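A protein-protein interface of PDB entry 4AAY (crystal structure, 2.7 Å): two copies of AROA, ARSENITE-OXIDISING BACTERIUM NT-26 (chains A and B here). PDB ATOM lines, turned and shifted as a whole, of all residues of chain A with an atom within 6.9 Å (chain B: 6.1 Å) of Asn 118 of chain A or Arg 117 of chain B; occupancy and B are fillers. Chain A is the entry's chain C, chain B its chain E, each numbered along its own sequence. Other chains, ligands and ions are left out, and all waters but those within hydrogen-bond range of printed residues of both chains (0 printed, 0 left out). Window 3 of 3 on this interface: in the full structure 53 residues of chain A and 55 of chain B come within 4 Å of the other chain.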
ATOM      1  N   ARG A   5      25.676  40.435  15.185  1.00  0.00           N
ATOM      2  CA  ARG A   5      25.994  39.249  14.384  1.00  0.00           C
ATOM      3  C   ARG A   5      27.211  39.427  13.518  1.00  0.00           C
ATOM      4  O   ARG A   5      27.842  38.450  13.157  1.00  0.00           O
ATOM      5  CB  ARG A   5      24.816  38.868  13.505  1.00  0.00           C
ATOM      6  CG  ARG A   5      23.590  38.423  14.275  1.00  0.00           C
ATOM      7  CD  ARG A   5      22.447  38.186  13.322  1.00  0.00           C
ATOM      8  NE  ARG A   5      21.249  37.755  14.023  1.00  0.00           N
ATOM      9  CZ  ARG A   5      20.440  38.558  14.703  1.00  0.00           C
ATOM     10  NH1 ARG A   5      20.694  39.859  14.795  1.00  0.00           N
ATOM     11  NH2 ARG A   5      19.367  38.056  15.301  1.00  0.00           N
ATOM     12  N   ASN A  75      19.210  31.621   6.483  1.00  0.00           N
ATOM     13  CA  ASN A  75      19.994  30.491   7.005  1.00  0.00           C
ATOM     14  C   ASN A  75      20.348  29.544   5.874  1.00  0.00           C
ATOM     15  O   ASN A  75      19.979  29.792   4.722  1.00  0.00           O
ATOM     16  CB  ASN A  75      19.232  29.753   8.119  1.00  0.00           C
ATOM     17  CG  ASN A  75      20.158  29.111   9.139  1.00  0.00           C
ATOM     18  OD1 ASN A  75      21.324  28.858   8.872  1.00  0.00           O
ATOM     19  ND2 ASN A  75      19.633  28.836  10.311  1.00  0.00           N
ATOM     20  N   VAL A  76      21.090  28.485   6.193  1.00  0.00           N
ATOM     21  CA  VAL A  76      21.343  27.389   5.249  1.00  0.00           C
ATOM     22  C   VAL A  76      20.821  26.111   5.870  1.00  0.00           C
ATOM     23  O   VAL A  76      21.192  25.781   6.984  1.00  0.00           O
ATOM     24  CB  VAL A  76      22.839  27.227   4.920  1.00  0.00           C
ATOM     25  CG1 VAL A  76      23.069  26.023   4.014  1.00  0.00           C
ATOM     26  CG2 VAL A  76      23.384  28.495   4.308  1.00  0.00           C
ATOM     27  N   SER A 112      16.006  27.875  12.909  1.00  0.00           N
ATOM     28  CA  SER A 112      15.939  26.575  12.244  1.00  0.00           C
ATOM     29  C   SER A 112      17.263  25.846  12.449  1.00  0.00           C
ATOM     30  O   SER A 112      18.277  26.455  12.786  1.00  0.00           O
ATOM     31  CB  SER A 112      15.691  26.744  10.743  1.00  0.00           C
ATOM     32  OG  SER A 112      14.568  27.555  10.483  1.00  0.00           O
ATOM     33  N   PHE A 113      17.248  24.543  12.219  1.00  0.00           N
ATOM     34  CA  PHE A 113      18.429  23.717  12.346  1.00  0.00           C
ATOM     35  C   PHE A 113      19.326  23.862  11.124  1.00  0.00           C
ATOM     36  O   PHE A 113      18.880  23.639  10.005  1.00  0.00           O
ATOM     37  CB  PHE A 113      18.003  22.263  12.493  1.00  0.00           C
ATOM     38  CG  PHE A 113      19.145  21.302  12.634  1.00  0.00           C
ATOM     39  CD1 PHE A 113      19.833  21.199  13.833  1.00  0.00           C
ATOM     40  CD2 PHE A 113      19.518  20.484  11.577  1.00  0.00           C
ATOM     41  CE1 PHE A 113      20.878  20.296  13.978  1.00  0.00           C
ATOM     42  CE2 PHE A 113      20.551  19.581  11.710  1.00  0.00           C
ATOM     43  CZ  PHE A 113      21.239  19.486  12.913  1.00  0.00           C
ATOM     44  N   SER A 114      20.589  24.209  11.358  1.00  0.00           N
ATOM     45  CA  SER A 114      21.614  24.271  10.306  1.00  0.00           C
ATOM     46  C   SER A 114      22.947  23.690  10.767  1.00  0.00           C
ATOM     47  O   SER A 114      23.583  24.243  11.665  1.00  0.00           O
ATOM     48  CB  SER A 114      21.854  25.717   9.887  1.00  0.00           C
ATOM     49  OG  SER A 114      22.945  25.835   8.975  1.00  0.00           O
ATOM     50  N   GLU A 115      23.374  22.581  10.158  1.00  0.00           N
ATOM     51  CA  GLU A 115      24.753  22.085  10.341  1.00  0.00           C
ATOM     52  C   GLU A 115      25.769  23.048   9.730  1.00  0.00           C
ATOM     53  O   GLU A 115      26.868  23.198  10.242  1.00  0.00           O
ATOM     54  CB  GLU A 115      24.960  20.688   9.731  1.00  0.00           C
ATOM     55  CG  GLU A 115      24.042  19.595  10.287  1.00  0.00           C
ATOM     56  CD  GLU A 115      24.648  18.181  10.229  1.00  0.00           C
ATOM     57  OE1 GLU A 115      25.648  17.971   9.481  1.00  0.00           O
ATOM     58  OE2 GLU A 115      24.119  17.290  10.953  1.00  0.00           O
ATOM     59  N   ALA A 116      25.401  23.697   8.638  1.00  0.00           N
ATOM     60  CA  ALA A 116      26.328  24.556   7.930  1.00  0.00           C
ATOM     61  C   ALA A 116      26.679  25.799   8.747  1.00  0.00           C
ATOM     62  O   ALA A 116      27.847  26.144   8.887  1.00  0.00           O
ATOM     63  CB  ALA A 116      25.778  24.939   6.572  1.00  0.00           C
ATOM     64  N   ARG A 117      25.676  26.462   9.298  1.00  0.00           N
ATOM     65  CA  ARG A 117      25.905  27.716  10.017  1.00  0.00           C
ATOM     66  C   ARG A 117      25.759  27.568  11.526  1.00  0.00           C
ATOM     67  O   ARG A 117      25.761  28.552  12.255  1.00  0.00           O
ATOM     68  CB  ARG A 117      24.983  28.797   9.459  1.00  0.00           C
ATOM     69  CG  ARG A 117      25.229  29.032   7.979  1.00  0.00           C
ATOM     70  CD  ARG A 117      24.332  30.107   7.394  1.00  0.00           C
ATOM     71  NE  ARG A 117      24.768  31.445   7.771  1.00  0.00           N
ATOM     72  CZ  ARG A 117      24.111  32.257   8.598  1.00  0.00           C
ATOM     73  NH1 ARG A 117      22.943  31.910   9.161  1.00  0.00           N
ATOM     74  NH2 ARG A 117      24.624  33.459   8.852  1.00  0.00           N
ATOM     75  N   ASN A 118      25.662  26.323  11.987  1.00  0.00           N
ATOM     76  CA  ASN A 118      25.659  25.983  13.416  1.00  0.00           C
ATOM     77  C   ASN A 118      24.541  26.634  14.249  1.00  0.00           C
ATOM     78  O   ASN A 118      24.758  27.037  15.377  1.00  0.00           O
ATOM     79  CB  ASN A 118      27.031  26.262  14.023  1.00  0.00           C
ATOM     80  CG  ASN A 118      28.021  25.135  13.766  1.00  0.00           C
ATOM     81  OD1 ASN A 118      28.891  25.253  12.897  1.00  0.00           O
ATOM     82  ND2 ASN A 118      27.893  24.031  14.525  1.00  0.00           N
ATOM     83  N   THR A 119      23.340  26.706  13.694  1.00  0.00           N
ATOM     84  CA  THR A 119      22.174  27.177  14.445  1.00  0.00           C
ATOM     85  C   THR A 119      21.386  25.993  15.050  1.00  0.00           C
ATOM     86  O   THR A 119      21.119  24.982  14.389  1.00  0.00           O
ATOM     87  CB  THR A 119      21.228  28.051  13.582  1.00  0.00           C
ATOM     88  OG1 THR A 119      20.776  27.306  12.437  1.00  0.00           O
ATOM     89  CG2 THR A 119      21.932  29.321  13.129  1.00  0.00           C
ATOM     90  N   GLN A 120      21.020  26.150  16.314  1.00  0.00           N
ATOM     91  CA  GLN A 120      20.188  25.195  17.029  1.00  0.00           C
ATOM     92  C   GLN A 120      20.746  23.768  17.033  1.00  0.00           C
ATOM     93  O   GLN A 120      20.025  22.809  16.789  1.00  0.00           O
ATOM     94  CB  GLN A 120      18.759  25.235  16.495  1.00  0.00           C
ATOM     95  CG  GLN A 120      18.079  26.586  16.666  1.00  0.00           C
ATOM     96  CD  GLN A 120      17.756  26.937  18.103  1.00  0.00           C
ATOM     97  OE1 GLN A 120      17.526  26.051  18.939  1.00  0.00           O
ATOM     98  NE2 GLN A 120      17.730  28.230  18.400  1.00  0.00           N
ATOM     99  N   GLN A 121      22.027  23.633  17.352  1.00  0.00           N
ATOM    100  CA  GLN A 121      22.675  22.304  17.477  1.00  0.00           C
ATOM    101  C   GLN A 121      22.064  21.524  18.622  1.00  0.00           C
ATOM    102  O   GLN A 121      22.258  20.329  18.707  1.00  0.00           O
ATOM    103  CB  GLN A 121      24.215  22.375  17.749  1.00  0.00           C
ATOM    104  CG  GLN A 121      25.184  22.031  16.596  1.00  0.00           C
ATOM    105  CD  GLN A 121      26.177  20.910  16.987  1.00  0.00           C
ATOM    106  OE1 GLN A 121      25.789  19.870  17.542  1.00  0.00           O
ATOM    107  NE2 GLN A 121      27.462  21.120  16.691  1.00  0.00           N
ATOM    108  N   GLU A 733      19.108  28.913  22.848  1.00  0.00           N
ATOM    109  CA  GLU A 733      20.250  28.784  21.926  1.00  0.00           C
ATOM    110  C   GLU A 733      20.291  29.920  20.875  1.00  0.00           C
ATOM    111  O   GLU A 733      20.865  29.777  19.807  1.00  0.00           O
ATOM    112  CB  GLU A 733      20.283  27.387  21.271  1.00  0.00           C
ATOM    113  CG  GLU A 733      21.394  26.489  21.793  1.00  0.00           C
ATOM    114  CD  GLU A 733      22.127  25.750  20.657  1.00  0.00           C
ATOM    115  OE1 GLU A 733      21.491  25.013  19.879  1.00  0.00           O
ATOM    116  OE2 GLU A 733      23.352  25.936  20.521  1.00  0.00           O
ATOM    117  N   ILE B   7      32.170  25.963   2.993  1.00  0.00           N
ATOM    118  CA  ILE B   7      32.865  27.248   3.091  1.00  0.00           C
ATOM    119  C   ILE B   7      33.773  27.400   1.858  1.00  0.00           C
ATOM    120  O   ILE B   7      34.829  26.802   1.767  1.00  0.00           O
ATOM    121  CB  ILE B   7      33.636  27.344   4.417  1.00  0.00           C
ATOM    122  CG1 ILE B   7      32.655  27.372   5.596  1.00  0.00           C
ATOM    123  CG2 ILE B   7      34.483  28.581   4.496  1.00  0.00           C
ATOM    124  CD1 ILE B   7      33.306  27.418   6.976  1.00  0.00           C
ATOM    125  N   LEU B  10      37.922  31.827   2.614  1.00  0.00           N
ATOM    126  CA  LEU B  10      38.234  32.261   3.948  1.00  0.00           C
ATOM    127  C   LEU B  10      38.867  33.633   3.864  1.00  0.00           C
ATOM    128  O   LEU B  10      39.577  33.931   2.922  1.00  0.00           O
ATOM    129  CB  LEU B  10      39.191  31.267   4.633  1.00  0.00           C
ATOM    130  CG  LEU B  10      38.719  29.832   4.915  1.00  0.00           C
ATOM    131  CD1 LEU B  10      39.907  29.002   5.391  1.00  0.00           C
ATOM    132  CD2 LEU B  10      37.578  29.786   5.944  1.00  0.00           C
ATOM    133  N   PRO B  71      39.537  25.578   6.690  1.00  0.00           N
ATOM    134  CA  PRO B  71      38.433  26.168   7.443  1.00  0.00           C
ATOM    135  C   PRO B  71      38.479  25.927   8.958  1.00  0.00           C
ATOM    136  O   PRO B  71      38.175  26.832   9.723  1.00  0.00           O
ATOM    137  CB  PRO B  71      37.208  25.477   6.858  1.00  0.00           C
ATOM    138  CG  PRO B  71      37.602  25.112   5.484  1.00  0.00           C
ATOM    139  CD  PRO B  71      39.073  24.870   5.489  1.00  0.00           C
ATOM    140  N   TYR B  74      40.256  28.462  11.015  1.00  0.00           N
ATOM    141  CA  TYR B  74      39.692  29.823  11.016  1.00  0.00           C
ATOM    142  C   TYR B  74      38.469  29.930  11.912  1.00  0.00           C
ATOM    143  O   TYR B  74      37.649  29.022  11.953  1.00  0.00           O
ATOM    144  CB  TYR B  74      39.261  30.241   9.610  1.00  0.00           C
ATOM    145  CG  TYR B  74      38.485  31.540   9.615  1.00  0.00           C
ATOM    146  CD1 TYR B  74      39.140  32.758   9.658  1.00  0.00           C
ATOM    147  CD2 TYR B  74      37.100  31.547   9.602  1.00  0.00           C
ATOM    148  CE1 TYR B  74      38.432  33.950   9.682  1.00  0.00           C
ATOM    149  CE2 TYR B  74      36.386  32.724   9.621  1.00  0.00           C
ATOM    150  CZ  TYR B  74      37.061  33.926   9.664  1.00  0.00           C
ATOM    151  OH  TYR B  74      36.363  35.114   9.691  1.00  0.00           O
ATOM    152  N   ASN B  75      38.344  31.054  12.614  1.00  0.00           N
ATOM    153  CA  ASN B  75      37.144  31.363  13.397  1.00  0.00           C
ATOM    154  C   ASN B  75      37.084  32.857  13.685  1.00  0.00           C
ATOM    155  O   ASN B  75      37.976  33.601  13.249  1.00  0.00           O
ATOM    156  CB  ASN B  75      37.119  30.560  14.697  1.00  0.00           C
ATOM    157  CG  ASN B  75      35.705  30.276  15.190  1.00  0.00           C
ATOM    158  OD1 ASN B  75      34.747  30.931  14.770  1.00  0.00           O
ATOM    159  ND2 ASN B  75      35.574  29.300  16.070  1.00  0.00           N
ATOM    160  N   VAL B  76      36.010  33.299  14.342  1.00  0.00           N
ATOM    161  CA  VAL B  76      35.914  34.667  14.852  1.00  0.00           C
ATOM    162  C   VAL B  76      35.703  34.607  16.346  1.00  0.00           C
ATOM    163  O   VAL B  76      34.804  33.933  16.813  1.00  0.00           O
ATOM    164  CB  VAL B  76      34.759  35.472  14.230  1.00  0.00           C
ATOM    165  CG1 VAL B  76      34.595  36.807  14.947  1.00  0.00           C
ATOM    166  CG2 VAL B  76      35.019  35.717  12.751  1.00  0.00           C
ATOM    167  N   GLU B 110      38.308  26.107  15.147  1.00  0.00           N
ATOM    168  CA  GLU B 110      36.925  25.646  15.004  1.00  0.00           C
ATOM    169  C   GLU B 110      36.344  25.091  16.301  1.00  0.00           C
ATOM    170  O   GLU B 110      35.126  25.042  16.458  1.00  0.00           O
ATOM    171  CB  GLU B 110      36.905  24.571  13.927  1.00  0.00           C
ATOM    172  CG  GLU B 110      35.579  23.894  13.676  1.00  0.00           C
ATOM    173  CD  GLU B 110      35.608  23.070  12.405  1.00  0.00           C
ATOM    174  OE1 GLU B 110      35.432  23.677  11.312  1.00  0.00           O
ATOM    175  OE2 GLU B 110      35.853  21.832  12.502  1.00  0.00           O
ATOM    176  N   SER B 114      32.985  30.801  19.770  1.00  0.00           N
ATOM    177  CA  SER B 114      32.580  31.943  18.947  1.00  0.00           C
ATOM    178  C   SER B 114      31.073  32.189  19.007  1.00  0.00           C
ATOM    179  O   SER B 114      30.292  31.372  18.528  1.00  0.00           O
ATOM    180  CB  SER B 114      32.972  31.698  17.487  1.00  0.00           C
ATOM    181  OG  SER B 114      32.473  32.710  16.609  1.00  0.00           O
ATOM    182  N   GLU B 115      30.672  33.328  19.562  1.00  0.00           N
ATOM    183  CA  GLU B 115      29.285  33.805  19.417  1.00  0.00           C
ATOM    184  C   GLU B 115      28.970  34.172  17.966  1.00  0.00           C
ATOM    185  O   GLU B 115      27.841  33.994  17.501  1.00  0.00           O
ATOM    186  CB  GLU B 115      28.991  35.026  20.299  1.00  0.00           C
ATOM    187  CG  GLU B 115      29.235  34.816  21.794  1.00  0.00           C
ATOM    188  CD  GLU B 115      28.382  35.719  22.689  1.00  0.00           C
ATOM    189  OE1 GLU B 115      27.807  36.732  22.185  1.00  0.00           O
ATOM    190  OE2 GLU B 115      28.257  35.388  23.910  1.00  0.00           O
ATOM    191  N   ALA B 116      29.959  34.678  17.247  1.00  0.00           N
ATOM    192  CA  ALA B 116      29.745  35.150  15.881  1.00  0.00           C
ATOM    193  C   ALA B 116      29.409  34.000  14.922  1.00  0.00           C
ATOM    194  O   ALA B 116      28.442  34.062  14.170  1.00  0.00           O
ATOM    195  CB  ALA B 116      30.963  35.903  15.405  1.00  0.00           C
ATOM    196  N   ARG B 117      30.193  32.935  14.987  1.00  0.00           N
ATOM    197  CA  ARG B 117      30.027  31.804  14.072  1.00  0.00           C
ATOM    198  C   ARG B 117      29.440  30.553  14.746  1.00  0.00           C
ATOM    199  O   ARG B 117      29.400  29.482  14.142  1.00  0.00           O
ATOM    200  CB  ARG B 117      31.360  31.501  13.384  1.00  0.00           C
ATOM    201  CG  ARG B 117      31.867  32.696  12.599  1.00  0.00           C
ATOM    202  CD  ARG B 117      33.190  32.433  11.906  1.00  0.00           C
ATOM    203  NE  ARG B 117      33.013  31.623  10.706  1.00  0.00           N
ATOM    204  CZ  ARG B 117      33.428  30.365  10.569  1.00  0.00           C
ATOM    205  NH1 ARG B 117      34.076  29.726  11.561  1.00  0.00           N
ATOM    206  NH2 ARG B 117      33.209  29.742   9.418  1.00  0.00           N
ATOM    207  N   ASN B 118      28.966  30.722  15.975  1.00  0.00           N
ATOM    208  CA  ASN B 118      28.240  29.687  16.706  1.00  0.00           C
ATOM    209  C   ASN B 118      29.012  28.372  16.921  1.00  0.00           C
ATOM    210  O   ASN B 118      28.442  27.290  16.848  1.00  0.00           O
ATOM    211  CB  ASN B 118      26.879  29.409  16.032  1.00  0.00           C
ATOM    212  CG  ASN B 118      25.806  30.410  16.425  1.00  0.00           C
ATOM    213  OD1 ASN B 118      25.532  31.357  15.695  1.00  0.00           O
ATOM    214  ND2 ASN B 118      25.190  30.196  17.598  1.00  0.00           N
ATOM    215  N   THR B 119      30.301  28.471  17.207  1.00  0.00           N
ATOM    216  CA  THR B 119      31.093  27.293  17.559  1.00  0.00           C
ATOM    217  C   THR B 119      31.169  27.106  19.097  1.00  0.00           C
ATOM    218  O   THR B 119      31.392  28.052  19.857  1.00  0.00           O
ATOM    219  CB  THR B 119      32.515  27.352  16.960  1.00  0.00           C
ATOM    220  OG1 THR B 119      33.198  28.520  17.442  1.00  0.00           O
ATOM    221  CG2 THR B 119      32.466  27.351  15.408  1.00  0.00           C
ATOM    222  N   GLN B 121      28.964  26.474  21.518  1.00  0.00           N
ATOM    223  CA  GLN B 121      28.013  27.168  22.386  1.00  0.00           C
ATOM    224  C   GLN B 121      27.743  26.381  23.668  1.00  0.00           C
ATOM    225  O   GLN B 121      27.206  26.920  24.620  1.00  0.00           O
ATOM    226  CB  GLN B 121      26.712  27.457  21.642  1.00  0.00           C
ATOM    227  CG  GLN B 121      26.854  28.544  20.581  1.00  0.00           C
ATOM    228  CD  GLN B 121      27.463  29.843  21.119  1.00  0.00           C
ATOM    229  OE1 GLN B 121      26.804  30.616  21.855  1.00  0.00           O
ATOM    230  NE2 GLN B 121      28.737  30.090  20.754  1.00  0.00           N
ATOM    231  N   GLU B 733      30.486  18.555  20.094  1.00  0.00           N
ATOM    232  CA  GLU B 733      29.891  19.721  19.419  1.00  0.00           C
ATOM    233  C   GLU B 733      30.646  20.076  18.107  1.00  0.00           C
ATOM    234  O   GLU B 733      30.603  21.200  17.628  1.00  0.00           O
ATOM    235  CB  GLU B 733      29.764  20.934  20.369  1.00  0.00           C
ATOM    236  CG  GLU B 733      28.332  21.212  20.815  1.00  0.00           C
ATOM    237  CD  GLU B 733      27.938  22.709  20.948  1.00  0.00           C
ATOM    238  OE1 GLU B 733      28.442  23.560  20.188  1.00  0.00           O
ATOM    239  OE2 GLU B 733      27.066  23.054  21.796  1.00  0.00           O
ATOM    240  N   ASP B 735      30.884  18.807  14.198  1.00  0.00           N
ATOM    241  CA  ASP B 735      30.190  17.968  13.232  1.00  0.00           C
ATOM    242  C   ASP B 735      31.126  17.015  12.476  1.00  0.00           C
ATOM    243  O   ASP B 735      30.749  15.892  12.176  1.00  0.00           O
ATOM    244  CB  ASP B 735      29.397  18.838  12.258  1.00  0.00           C
ATOM    245  CG  ASP B 735      28.182  19.493  12.910  1.00  0.00           C
ATOM    246  OD1 ASP B 735      27.471  18.785  13.672  1.00  0.00           O
ATOM    247  OD2 ASP B 735      27.928  20.701  12.657  1.00  0.00           O
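NE2 of Gln 121 of chain A lies within hydrogen-bond range of O of Glu 733 of chain B (3.3 Å).
The backbone NH (N) of Gln 121 of chain A is in hydrogen-bond range of the side-chain carboxylate (OE1) of Glu 733 of chain A (2.9 Å).
The side-chain amide oxygen of Asn 75 of chain B lies within hydrogen-bond range of the guanidinium group of Arg 117 of chain B (3.5 Å).
The backbone NH (N) of Arg 117 of chain B is in hydrogen-bond range of the side-chain hydroxyl (OG) of Ser 114 of chain B (2.8 Å).
O of Ser 114 of chain B lies within hydrogen-bond range of NE2 of Gln 121 of chain B.
The backbone carbonyl oxygen (O) of Thr 119 of chain B lies within hydrogen-bond range of the side-chain amide nitrogen (NE2) of Gln 121 of chain B, 3.5 Å away.
OE1 of Glu 733 of chain B sits at hydrogen-bond distance from N of Gln 121 of chain B (3.2 Å).
Among the printed residues, merely in contact across the chains: Asn 118 of chain A with Asn 118 of chain B, Glu 115 of chain A with Asp 735 of chain B, Gln 121 of chain A with Asp 735 of chain B, Asn 118 of chain A with Asp 735 of chain B, Glu 733 of chain A with Gln 121 of chain B and Asn 118 of chain A with Arg 117 of chain B.
Of the printed residues of chain B, Glu 115 of chain A touches Asp 735.
Of the printed residues of chain B, Asn 118 of chain A touches Arg 117, Asn 118 and Asp 735.
Printed residues of chain B within 4 Å of Glu 733 of chain A: Gln 121 (3.9 Å).
Ser 114 of chain B touches none of the printed residues of chain A.
Glu 115 of chain B touches none of the printed residues of chain A.
Of the printed residues of chain A, Gln 121 of chain B touches Glu 733.
Of the printed residues of chain A, Glu 733 of chain B touches Gln 121.
Of the printed residues of chain A, Asp 735 of chain B touches Glu 115 (3.6 Å), Asn 118 (3.8 Å) and Gln 121 (3.8 Å).
The nearest printed residue of chain B that does not touch Asn 118 of chain A is Thr 119 of chain B (4.8 Å).
The nearest printed residue of chain A that does not touch Arg 117 of chain B is Arg 117 of chain A (4.2 Å).
Of the 16 printed residues of chain B, 5 touch a printed residue of chain A.
Along chain B the printed residues that touch a printed residue of chain A span positions 117 to 735.
Among the printed residues, no Asp or Glu carboxylate lies within 4 Å of a Lys or Arg side-chain nitrogen of the other chain.
Asn 118 of chain A touches Arg 117 of chain B, but with the chains exchanged Arg 117 of chain A does not touch Asn 118 of chain B (4.03 Å).
Asn 118 of chain B touches its own counterpart, Asn 118 of chain A.
Gln 121 of chain A touches Glu 733 of chain B, and with the chains exchanged Glu 733 of chain A touches Gln 121 of chain B.
Positions printed for both chains: 75, 76, 114, 115, 116, 117, 118, 119, 121 and 733.
Of the 7 pairs that touch across the chains among the printed residues, 3 have their exchanged pair printed and touching as well.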
